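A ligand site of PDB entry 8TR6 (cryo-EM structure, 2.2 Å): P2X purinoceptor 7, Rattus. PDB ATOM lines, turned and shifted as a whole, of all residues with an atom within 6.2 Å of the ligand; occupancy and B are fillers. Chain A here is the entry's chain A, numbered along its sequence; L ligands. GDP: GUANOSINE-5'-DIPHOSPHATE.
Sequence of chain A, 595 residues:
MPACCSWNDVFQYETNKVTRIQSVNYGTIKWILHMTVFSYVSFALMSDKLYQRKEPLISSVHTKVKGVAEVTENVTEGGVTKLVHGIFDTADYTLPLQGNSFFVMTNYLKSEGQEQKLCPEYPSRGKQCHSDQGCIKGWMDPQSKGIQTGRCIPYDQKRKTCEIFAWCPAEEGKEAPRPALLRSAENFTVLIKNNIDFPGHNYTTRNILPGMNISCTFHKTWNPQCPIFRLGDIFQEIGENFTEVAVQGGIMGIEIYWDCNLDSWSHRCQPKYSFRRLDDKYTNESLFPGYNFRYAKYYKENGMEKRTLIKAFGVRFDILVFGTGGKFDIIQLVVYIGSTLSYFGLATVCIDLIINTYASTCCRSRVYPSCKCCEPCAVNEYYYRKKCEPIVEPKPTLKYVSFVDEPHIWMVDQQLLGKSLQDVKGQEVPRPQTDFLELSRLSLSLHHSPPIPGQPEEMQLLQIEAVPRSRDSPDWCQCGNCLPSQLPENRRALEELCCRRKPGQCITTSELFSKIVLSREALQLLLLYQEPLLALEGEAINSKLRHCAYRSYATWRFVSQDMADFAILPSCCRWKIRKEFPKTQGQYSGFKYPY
The backbone carbonyl oxygen (O) of Leu 569 lies within hydrogen-bond range of the guanidinium group (NH2) of Arg 574. The guanidinium group (NE) of Arg 578 is in hydrogen-bond range of the side-chain hydroxyl (OH) of Tyr 550, at 2.8 Å. The side-chain carboxylate (OE2) of Glu 495 is in salt-bridge range of the guanidinium group (NH2) of Arg 578 (3.6 Å). NH1 of Arg 574 lies within salt-bridge range of OE2 of Glu 495 (3.6 Å). N of Lys 583 is in hydrogen-bond range of OH of Tyr 588 (2.9 Å). The backbone carbonyl oxygen (O) of Gln 587 lies within hydrogen-bond range of the side-chain amino group (NZ) of Lys 583.
Merely in contact with the ligand: Asp 565, Ile 568, Gln 587 and Tyr 588. Within 4 Å of the ligand: Arg 546, His 547, Tyr 550, Ala 564, Asp 565, Ala 567, Ile 568, Leu 569, Arg 574, Arg 578, Lys 583, Gln 587, Tyr 588, Ser 589, Gly 590, Phe 591 and Lys 592. Along chain A the residues within 4 Å of the ligand span positions 546 to 592.
NZ of Lys 583 lies within salt-bridge range of O3B of the ligand. An oxygen (O6) of the ligand sits at hydrogen-bond distance from the backbone NH of Leu 569 (2.8 Å). O6 of the ligand sits at hydrogen-bond distance from NH2 of Arg 574 (2.7 Å). An oxygen (O2') of the ligand lies close to the backbone NH (N) of Lys 592. The side-chain hydroxyl of Ser 589 sits at hydrogen-bond distance from an oxygen (O3B) of the ligand, at 3.1 Å. An oxygen (O2A) of the ligand sits at hydrogen-bond distance from the backbone NH of Gly 590 (3.0 Å). The backbone carbonyl oxygen of Ala 567 is in hydrogen-bond range of a nitrogen (N1) of the ligand, at 2.8 Å. N2 of the ligand lies within hydrogen-bond range of O of Ala 564. The guanidinium group (NE) of Arg 546 lies within salt-bridge range of an oxygen (O1A) of the ligand (2.9 Å). O1A of the ligand lies within hydrogen-bond range of OH of Tyr 550. The backbone NH (N) of Ser 589 sits at hydrogen-bond distance from an oxygen (O3A) of the ligand (2.8 Å). A ring nitrogen (NE2) of His 547 lies within hydrogen-bond range of an oxygen (O2B) of the ligand. The guanidinium group (NH2) of Arg 578 lies within salt-bridge range of an oxygen (O2A) of the ligand (2.9 Å). A nitrogen (N7) of the ligand lies within hydrogen-bond range of the backbone NH (N) of Phe 591, 3.3 Å away.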
ATOM      1  N   GLU A 495      -6.789  30.695  10.026  1.00  0.00           N
ATOM      2  CA  GLU A 495      -5.905  29.814   9.290  1.00  0.00           C
ATOM      3  C   GLU A 495      -5.478  30.377   7.939  1.00  0.00           C
ATOM      4  O   GLU A 495      -4.702  29.723   7.236  1.00  0.00           O
ATOM      5  CB  GLU A 495      -6.578  28.453   9.094  1.00  0.00           C
ATOM      6  CG  GLU A 495      -6.528  27.557  10.308  1.00  0.00           C
ATOM      7  CD  GLU A 495      -6.988  26.137  10.019  1.00  0.00           C
ATOM      8  OE1 GLU A 495      -7.204  25.821   8.836  1.00  0.00           O
ATOM      9  OE2 GLU A 495      -7.139  25.352  10.976  1.00  0.00           O
ATOM     10  N   SER A 543      -2.408  11.709  16.152  1.00  0.00           N
ATOM     11  CA  SER A 543      -2.861  13.013  16.618  1.00  0.00           C
ATOM     12  C   SER A 543      -1.815  13.562  17.572  1.00  0.00           C
ATOM     13  O   SER A 543      -1.521  14.750  17.542  1.00  0.00           O
ATOM     14  CB  SER A 543      -4.217  12.900  17.322  1.00  0.00           C
ATOM     15  OG  SER A 543      -4.121  12.125  18.502  1.00  0.00           O
ATOM     16  N   ARG A 546       0.874  14.916  15.440  1.00  0.00           N
ATOM     17  CA  ARG A 546       0.470  16.169  14.809  1.00  0.00           C
ATOM     18  C   ARG A 546       0.599  17.331  15.791  1.00  0.00           C
ATOM     19  O   ARG A 546       1.126  18.399  15.454  1.00  0.00           O
ATOM     20  CB  ARG A 546      -0.963  16.045  14.291  1.00  0.00           C
ATOM     21  CG  ARG A 546      -1.352  17.112  13.289  1.00  0.00           C
ATOM     22  CD  ARG A 546      -2.673  16.800  12.609  1.00  0.00           C
ATOM     23  NE  ARG A 546      -3.681  16.297  13.544  1.00  0.00           N
ATOM     24  CZ  ARG A 546      -4.046  15.031  13.658  1.00  0.00           C
ATOM     25  NH1 ARG A 546      -3.506  14.080  12.917  1.00  0.00           N
ATOM     26  NH2 ARG A 546      -4.977  14.708  14.555  1.00  0.00           N
ATOM     27  N   HIS A 547       0.113  17.133  17.021  1.00  0.00           N
ATOM     28  CA  HIS A 547       0.217  18.183  18.035  1.00  0.00           C
ATOM     29  C   HIS A 547       1.674  18.461  18.386  1.00  0.00           C
ATOM     30  O   HIS A 547       2.060  19.620  18.588  1.00  0.00           O
ATOM     31  CB  HIS A 547      -0.566  17.784  19.281  1.00  0.00           C
ATOM     32  CG  HIS A 547      -2.020  17.526  19.016  1.00  0.00           C
ATOM     33  ND1 HIS A 547      -2.869  17.036  19.987  1.00  0.00           N
ATOM     34  CD2 HIS A 547      -2.773  17.693  17.911  1.00  0.00           C
ATOM     35  CE1 HIS A 547      -4.078  16.910  19.486  1.00  0.00           C
ATOM     36  NE2 HIS A 547      -4.052  17.298  18.219  1.00  0.00           N
ATOM     37  N   TYR A 550       3.104  20.584  15.667  1.00  0.00           N
ATOM     38  CA  TYR A 550       2.670  21.955  15.846  1.00  0.00           C
ATOM     39  C   TYR A 550       3.505  22.651  16.907  1.00  0.00           C
ATOM     40  O   TYR A 550       4.005  23.767  16.704  1.00  0.00           O
ATOM     41  CB  TYR A 550       1.186  22.005  16.223  1.00  0.00           C
ATOM     42  CG  TYR A 550       0.232  21.526  15.157  1.00  0.00           C
ATOM     43  CD1 TYR A 550       0.561  21.562  13.809  1.00  0.00           C
ATOM     44  CD2 TYR A 550      -1.017  21.032  15.507  1.00  0.00           C
ATOM     45  CE1 TYR A 550      -0.325  21.124  12.848  1.00  0.00           C
ATOM     46  CE2 TYR A 550      -1.906  20.600  14.552  1.00  0.00           C
ATOM     47  CZ  TYR A 550      -1.552  20.640  13.226  1.00  0.00           C
ATOM     48  OH  TYR A 550      -2.447  20.203  12.276  1.00  0.00           O
ATOM     49  N   ALA A 554       6.104  25.802  16.402  1.00  0.00           N
ATOM     50  CA  ALA A 554       5.875  27.035  17.153  1.00  0.00           C
ATOM     51  C   ALA A 554       7.084  27.392  17.997  1.00  0.00           C
ATOM     52  O   ALA A 554       7.487  28.563  18.043  1.00  0.00           O
ATOM     53  CB  ALA A 554       4.623  26.888  18.024  1.00  0.00           C
ATOM     54  N   MET A 563       4.953  32.888  23.511  1.00  0.00           N
ATOM     55  CA  MET A 563       4.501  33.182  22.153  1.00  0.00           C
ATOM     56  C   MET A 563       4.065  31.917  21.426  1.00  0.00           C
ATOM     57  O   MET A 563       3.088  31.939  20.668  1.00  0.00           O
ATOM     58  CB  MET A 563       5.607  33.887  21.376  1.00  0.00           C
ATOM     59  CG  MET A 563       5.781  35.355  21.740  1.00  0.00           C
ATOM     60  SD  MET A 563       6.795  36.250  20.562  1.00  0.00           S
ATOM     61  CE  MET A 563       8.406  35.547  20.889  1.00  0.00           C
ATOM     62  N   ALA A 564       4.779  30.804  21.644  1.00  0.00           N
ATOM     63  CA  ALA A 564       4.441  29.561  20.964  1.00  0.00           C
ATOM     64  C   ALA A 564       3.066  29.063  21.373  1.00  0.00           C
ATOM     65  O   ALA A 564       2.329  28.498  20.559  1.00  0.00           O
ATOM     66  CB  ALA A 564       5.499  28.497  21.253  1.00  0.00           C
ATOM     67  N   ASP A 565       2.698  29.255  22.646  1.00  0.00           N
ATOM     68  CA  ASP A 565       1.379  28.837  23.099  1.00  0.00           C
ATOM     69  C   ASP A 565       0.269  29.539  22.326  1.00  0.00           C
ATOM     70  O   ASP A 565      -0.796  28.957  22.090  1.00  0.00           O
ATOM     71  CB  ASP A 565       1.220  29.110  24.596  1.00  0.00           C
ATOM     72  CG  ASP A 565       1.906  28.066  25.452  1.00  0.00           C
ATOM     73  OD1 ASP A 565       2.726  27.293  24.907  1.00  0.00           O
ATOM     74  OD2 ASP A 565       1.631  28.017  26.669  1.00  0.00           O
ATOM     75  N   PHE A 566       0.498  30.787  21.907  1.00  0.00           N
ATOM     76  CA  PHE A 566      -0.480  31.563  21.170  1.00  0.00           C
ATOM     77  C   PHE A 566      -0.047  31.806  19.721  1.00  0.00           C
ATOM     78  O   PHE A 566      -0.652  32.640  19.043  1.00  0.00           O
ATOM     79  CB  PHE A 566      -0.743  32.892  21.866  1.00  0.00           C
ATOM     80  CG  PHE A 566      -1.495  32.753  23.153  1.00  0.00           C
ATOM     81  CD1 PHE A 566      -2.875  32.691  23.148  1.00  0.00           C
ATOM     82  CD2 PHE A 566      -0.823  32.681  24.352  1.00  0.00           C
ATOM     83  CE1 PHE A 566      -3.573  32.558  24.331  1.00  0.00           C
ATOM     84  CE2 PHE A 566      -1.522  32.548  25.535  1.00  0.00           C
ATOM     85  CZ  PHE A 566      -2.892  32.485  25.519  1.00  0.00           C
ATOM     86  N   ALA A 567       0.967  31.096  19.248  1.00  0.00           N
ATOM     87  CA  ALA A 567       1.395  31.245  17.866  1.00  0.00           C
ATOM     88  C   ALA A 567       0.360  30.629  16.927  1.00  0.00           C
ATOM     89  O   ALA A 567      -0.446  29.792  17.317  1.00  0.00           O
ATOM     90  CB  ALA A 567       2.760  30.603  17.656  1.00  0.00           C
ATOM     91  N   ILE A 568       0.386  31.074  15.675  1.00  0.00           N
ATOM     92  CA  ILE A 568      -0.495  30.567  14.639  1.00  0.00           C
ATOM     93  C   ILE A 568       0.376  29.997  13.525  1.00  0.00           C
ATOM     94  O   ILE A 568       1.224  30.704  12.973  1.00  0.00           O
ATOM     95  CB  ILE A 568      -1.440  31.649  14.090  1.00  0.00           C
ATOM     96  CG1 ILE A 568      -2.164  32.365  15.229  1.00  0.00           C
ATOM     97  CG2 ILE A 568      -2.449  31.038  13.126  1.00  0.00           C
ATOM     98  CD1 ILE A 568      -3.020  31.465  16.085  1.00  0.00           C
ATOM     99  N   LEU A 569       0.166  28.725  13.211  1.00  0.00           N
ATOM    100  CA  LEU A 569       0.953  28.074  12.180  1.00  0.00           C
ATOM    101  C   LEU A 569       0.498  28.530  10.800  1.00  0.00           C
ATOM    102  O   LEU A 569      -0.693  28.749  10.576  1.00  0.00           O
ATOM    103  CB  LEU A 569       0.834  26.563  12.287  1.00  0.00           C
ATOM    104  CG  LEU A 569       1.963  25.859  13.039  1.00  0.00           C
ATOM    105  CD1 LEU A 569       1.736  25.904  14.538  1.00  0.00           C
ATOM    106  CD2 LEU A 569       2.103  24.427  12.551  1.00  0.00           C
ATOM    107  N   PRO A 570       1.417  28.688   9.845  1.00  0.00           N
ATOM    108  CA  PRO A 570       1.007  28.972   8.468  1.00  0.00           C
ATOM    109  C   PRO A 570       0.205  27.824   7.894  1.00  0.00           C
ATOM    110  O   PRO A 570       0.358  26.664   8.283  1.00  0.00           O
ATOM    111  CB  PRO A 570       2.340  29.161   7.721  1.00  0.00           C
ATOM    112  CG  PRO A 570       3.325  29.476   8.776  1.00  0.00           C
ATOM    113  CD  PRO A 570       2.881  28.755   9.999  1.00  0.00           C
ATOM    114  N   ARG A 574       0.959  23.881   8.342  1.00  0.00           N
ATOM    115  CA  ARG A 574      -0.094  23.142   9.026  1.00  0.00           C
ATOM    116  C   ARG A 574      -0.585  21.984   8.180  1.00  0.00           C
ATOM    117  O   ARG A 574      -0.719  20.853   8.665  1.00  0.00           O
ATOM    118  CB  ARG A 574      -1.243  24.099   9.368  1.00  0.00           C
ATOM    119  CG  ARG A 574      -2.618  23.463   9.561  1.00  0.00           C
ATOM    120  CD  ARG A 574      -3.711  24.513   9.542  1.00  0.00           C
ATOM    121  NE  ARG A 574      -3.319  25.728  10.243  1.00  0.00           N
ATOM    122  CZ  ARG A 574      -3.407  25.891  11.554  1.00  0.00           C
ATOM    123  NH1 ARG A 574      -3.859  24.936  12.344  1.00  0.00           N
ATOM    124  NH2 ARG A 574      -3.018  27.051  12.087  1.00  0.00           N
ATOM    125  N   ARG A 578      -0.345  17.946   8.674  1.00  0.00           N
ATOM    126  CA  ARG A 578      -1.537  17.101   8.662  1.00  0.00           C
ATOM    127  C   ARG A 578      -1.411  15.995   7.617  1.00  0.00           C
ATOM    128  O   ARG A 578      -1.847  14.862   7.850  1.00  0.00           O
ATOM    129  CB  ARG A 578      -2.774  17.958   8.399  1.00  0.00           C
ATOM    130  CG  ARG A 578      -3.260  18.680   9.641  1.00  0.00           C
ATOM    131  CD  ARG A 578      -4.069  19.921   9.295  1.00  0.00           C
ATOM    132  NE  ARG A 578      -4.570  20.573  10.500  1.00  0.00           N
ATOM    133  CZ  ARG A 578      -5.429  21.580  10.500  1.00  0.00           C
ATOM    134  NH1 ARG A 578      -5.901  22.089   9.374  1.00  0.00           N
ATOM    135  NH2 ARG A 578      -5.814  22.100  11.664  1.00  0.00           N
ATOM    136  N   LYS A 583      -5.748  12.945   9.982  1.00  0.00           N
ATOM    137  CA  LYS A 583      -6.870  12.447  10.761  1.00  0.00           C
ATOM    138  C   LYS A 583      -7.756  11.600   9.852  1.00  0.00           C
ATOM    139  O   LYS A 583      -8.105  12.029   8.754  1.00  0.00           O
ATOM    140  CB  LYS A 583      -7.674  13.612  11.353  1.00  0.00           C
ATOM    141  CG  LYS A 583      -8.362  13.298  12.668  1.00  0.00           C
ATOM    142  CD  LYS A 583      -9.330  14.405  13.046  1.00  0.00           C
ATOM    143  CE  LYS A 583      -9.643  14.389  14.529  1.00  0.00           C
ATOM    144  NZ  LYS A 583     -10.411  15.603  14.934  1.00  0.00           N
ATOM    145  N   GLN A 587     -12.747  16.163  11.480  1.00  0.00           N
ATOM    146  CA  GLN A 587     -12.426  17.524  11.068  1.00  0.00           C
ATOM    147  C   GLN A 587     -11.490  18.153  12.090  1.00  0.00           C
ATOM    148  O   GLN A 587     -11.736  18.083  13.296  1.00  0.00           O
ATOM    149  CB  GLN A 587     -13.695  18.366  10.927  1.00  0.00           C
ATOM    150  CG  GLN A 587     -13.667  19.335   9.759  1.00  0.00           C
ATOM    151  CD  GLN A 587     -13.740  18.626   8.415  1.00  0.00           C
ATOM    152  OE1 GLN A 587     -13.804  17.404   8.347  1.00  0.00           O
ATOM    153  NE2 GLN A 587     -13.728  19.401   7.338  1.00  0.00           N
ATOM    154  N   TYR A 588     -10.392  18.762  11.621  1.00  0.00           N
ATOM    155  CA  TYR A 588      -9.404  19.335  12.540  1.00  0.00           C
ATOM    156  C   TYR A 588      -9.943  20.509  13.335  1.00  0.00           C
ATOM    157  O   TYR A 588     -10.513  21.439  12.765  1.00  0.00           O
ATOM    158  CB  TYR A 588      -8.154  19.797  11.790  1.00  0.00           C
ATOM    159  CG  TYR A 588      -7.391  18.693  11.102  1.00  0.00           C
ATOM    160  CD1 TYR A 588      -6.615  17.806  11.830  1.00  0.00           C
ATOM    161  CD2 TYR A 588      -7.454  18.537   9.724  1.00  0.00           C
ATOM    162  CE1 TYR A 588      -5.912  16.790  11.207  1.00  0.00           C
ATOM    163  CE2 TYR A 588      -6.759  17.524   9.094  1.00  0.00           C
ATOM    164  CZ  TYR A 588      -5.997  16.661   9.836  1.00  0.00           C
ATOM    165  OH  TYR A 588      -5.304  15.655   9.214  1.00  0.00           O
ATOM    166  N   SER A 589      -9.756  20.483  14.653  1.00  0.00           N
ATOM    167  CA  SER A 589     -10.226  21.563  15.512  1.00  0.00           C
ATOM    168  C   SER A 589      -9.492  22.852  15.221  1.00  0.00           C
ATOM    169  O   SER A 589     -10.095  23.917  15.187  1.00  0.00           O
ATOM    170  CB  SER A 589     -10.031  21.190  16.971  1.00  0.00           C
ATOM    171  OG  SER A 589     -10.838  20.082  17.328  1.00  0.00           O
ATOM    172  N   GLY A 590      -8.182  22.759  15.015  1.00  0.00           N
ATOM    173  CA  GLY A 590      -7.384  23.941  14.787  1.00  0.00           C
ATOM    174  C   GLY A 590      -6.926  24.567  16.086  1.00  0.00           C
ATOM    175  O   GLY A 590      -6.976  23.922  17.132  1.00  0.00           O
ATOM    176  N   PHE A 591      -6.387  25.783  16.005  1.00  0.00           N
ATOM    177  CA  PHE A 591      -5.852  26.436  17.201  1.00  0.00           C
ATOM    178  C   PHE A 591      -6.890  26.540  18.300  1.00  0.00           C
ATOM    179  O   PHE A 591      -8.055  26.844  18.028  1.00  0.00           O
ATOM    180  CB  PHE A 591      -5.322  27.827  16.858  1.00  0.00           C
ATOM    181  CG  PHE A 591      -4.733  28.551  18.031  1.00  0.00           C
ATOM    182  CD1 PHE A 591      -5.540  29.108  19.004  1.00  0.00           C
ATOM    183  CD2 PHE A 591      -3.356  28.663  18.163  1.00  0.00           C
ATOM    184  CE1 PHE A 591      -4.996  29.774  20.085  1.00  0.00           C
ATOM    185  CE2 PHE A 591      -2.805  29.326  19.251  1.00  0.00           C
ATOM    186  CZ  PHE A 591      -3.624  29.873  20.214  1.00  0.00           C
ATOM    187  N   LYS A 592      -6.472  26.297  19.532  1.00  0.00           N
ATOM    188  CA  LYS A 592      -7.381  26.395  20.659  1.00  0.00           C
ATOM    189  C   LYS A 592      -6.859  27.421  21.624  1.00  0.00           C
ATOM    190  O   LYS A 592      -5.676  27.423  21.959  1.00  0.00           O
ATOM    191  CB  LYS A 592      -7.490  25.046  21.366  1.00  0.00           C
ATOM    192  CG  LYS A 592      -8.480  25.057  22.521  1.00  0.00           C
ATOM    193  CD  LYS A 592      -8.603  23.688  23.170  1.00  0.00           C
ATOM    194  CE  LYS A 592      -9.581  23.739  24.333  1.00  0.00           C
ATOM    195  NZ  LYS A 592      -9.726  22.417  24.999  1.00  0.00           N
ATOM    196  N   TYR A 593      -7.738  28.297  22.084  1.00  0.00           N
ATOM    197  CA  TYR A 593      -7.334  29.271  23.072  1.00  0.00           C
ATOM    198  C   TYR A 593      -6.863  28.478  24.270  1.00  0.00           C
ATOM    199  O   TYR A 593      -7.622  27.689  24.838  1.00  0.00           O
ATOM    200  CB  TYR A 593      -8.525  30.150  23.419  1.00  0.00           C
ATOM    201  CG  TYR A 593      -8.303  31.163  24.520  1.00  0.00           C
ATOM    202  CD1 TYR A 593      -7.171  31.961  24.557  1.00  0.00           C
ATOM    203  CD2 TYR A 593      -9.259  31.357  25.496  1.00  0.00           C
ATOM    204  CE1 TYR A 593      -6.988  32.902  25.552  1.00  0.00           C
ATOM    205  CE2 TYR A 593      -9.096  32.289  26.493  1.00  0.00           C
ATOM    206  CZ  TYR A 593      -7.963  33.059  26.514  1.00  0.00           C
ATOM    207  OH  TYR A 593      -7.814  33.978  27.519  1.00  0.00           O
HETATM  208  PB  GDP L   1      -7.606  17.874  15.749  1.00  0.00           P
HETATM  209  O1B GDP L   1      -7.301  16.749  14.796  1.00  0.00           O
HETATM  210  O2B GDP L   1      -6.849  17.676  17.039  1.00  0.00           O
HETATM  211  O3B GDP L   1      -9.083  17.885  16.049  1.00  0.00           O
HETATM  212  O3A GDP L   1      -7.211  19.285  15.090  1.00  0.00           O
HETATM  213  PA  GDP L   1      -5.689  19.811  15.041  1.00  0.00           P
HETATM  214  O1A GDP L   1      -4.812  18.867  14.246  1.00  0.00           O
HETATM  215  O2A GDP L   1      -5.638  21.198  14.450  1.00  0.00           O
HETATM  216  O5' GDP L   1      -5.261  19.848  16.585  1.00  0.00           O
HETATM  217  C5' GDP L   1      -5.872  20.786  17.461  1.00  0.00           C
HETATM  218  C4' GDP L   1      -4.914  21.140  18.584  1.00  0.00           C
HETATM  219  O4' GDP L   1      -3.687  21.602  18.019  1.00  0.00           O
HETATM  220  C3' GDP L   1      -5.480  22.247  19.452  1.00  0.00           C
HETATM  221  O3' GDP L   1      -5.548  21.863  20.832  1.00  0.00           O
HETATM  222  C2' GDP L   1      -4.551  23.434  19.271  1.00  0.00           C
HETATM  223  O2' GDP L   1      -4.107  23.961  20.518  1.00  0.00           O
HETATM  224  C1' GDP L   1      -3.383  22.918  18.460  1.00  0.00           C
HETATM  225  N9  GDP L   1      -3.183  23.825  17.305  1.00  0.00           N
HETATM  226  C8  GDP L   1      -3.783  23.701  16.114  1.00  0.00           C
HETATM  227  N7  GDP L   1      -3.385  24.676  15.267  1.00  0.00           N
HETATM  228  C5  GDP L   1      -2.515  25.449  15.932  1.00  0.00           C
HETATM  229  C6  GDP L   1      -1.708  26.652  15.625  1.00  0.00           C
HETATM  230  O6  GDP L   1      -1.784  27.182  14.514  1.00  0.00           O
HETATM  231  N1  GDP L   1      -0.921  27.153  16.571  1.00  0.00           N
HETATM  232  C2  GDP L   1      -0.829  26.596  17.792  1.00  0.00           C
HETATM  233  N2  GDP L   1      -0.001  27.174  18.702  1.00  0.00           N
HETATM  234  N3  GDP L   1      -1.535  25.494  18.152  1.00  0.00           N
HETATM  235  C4  GDP L   1      -2.375  24.884  17.270  1.00  0.00           C
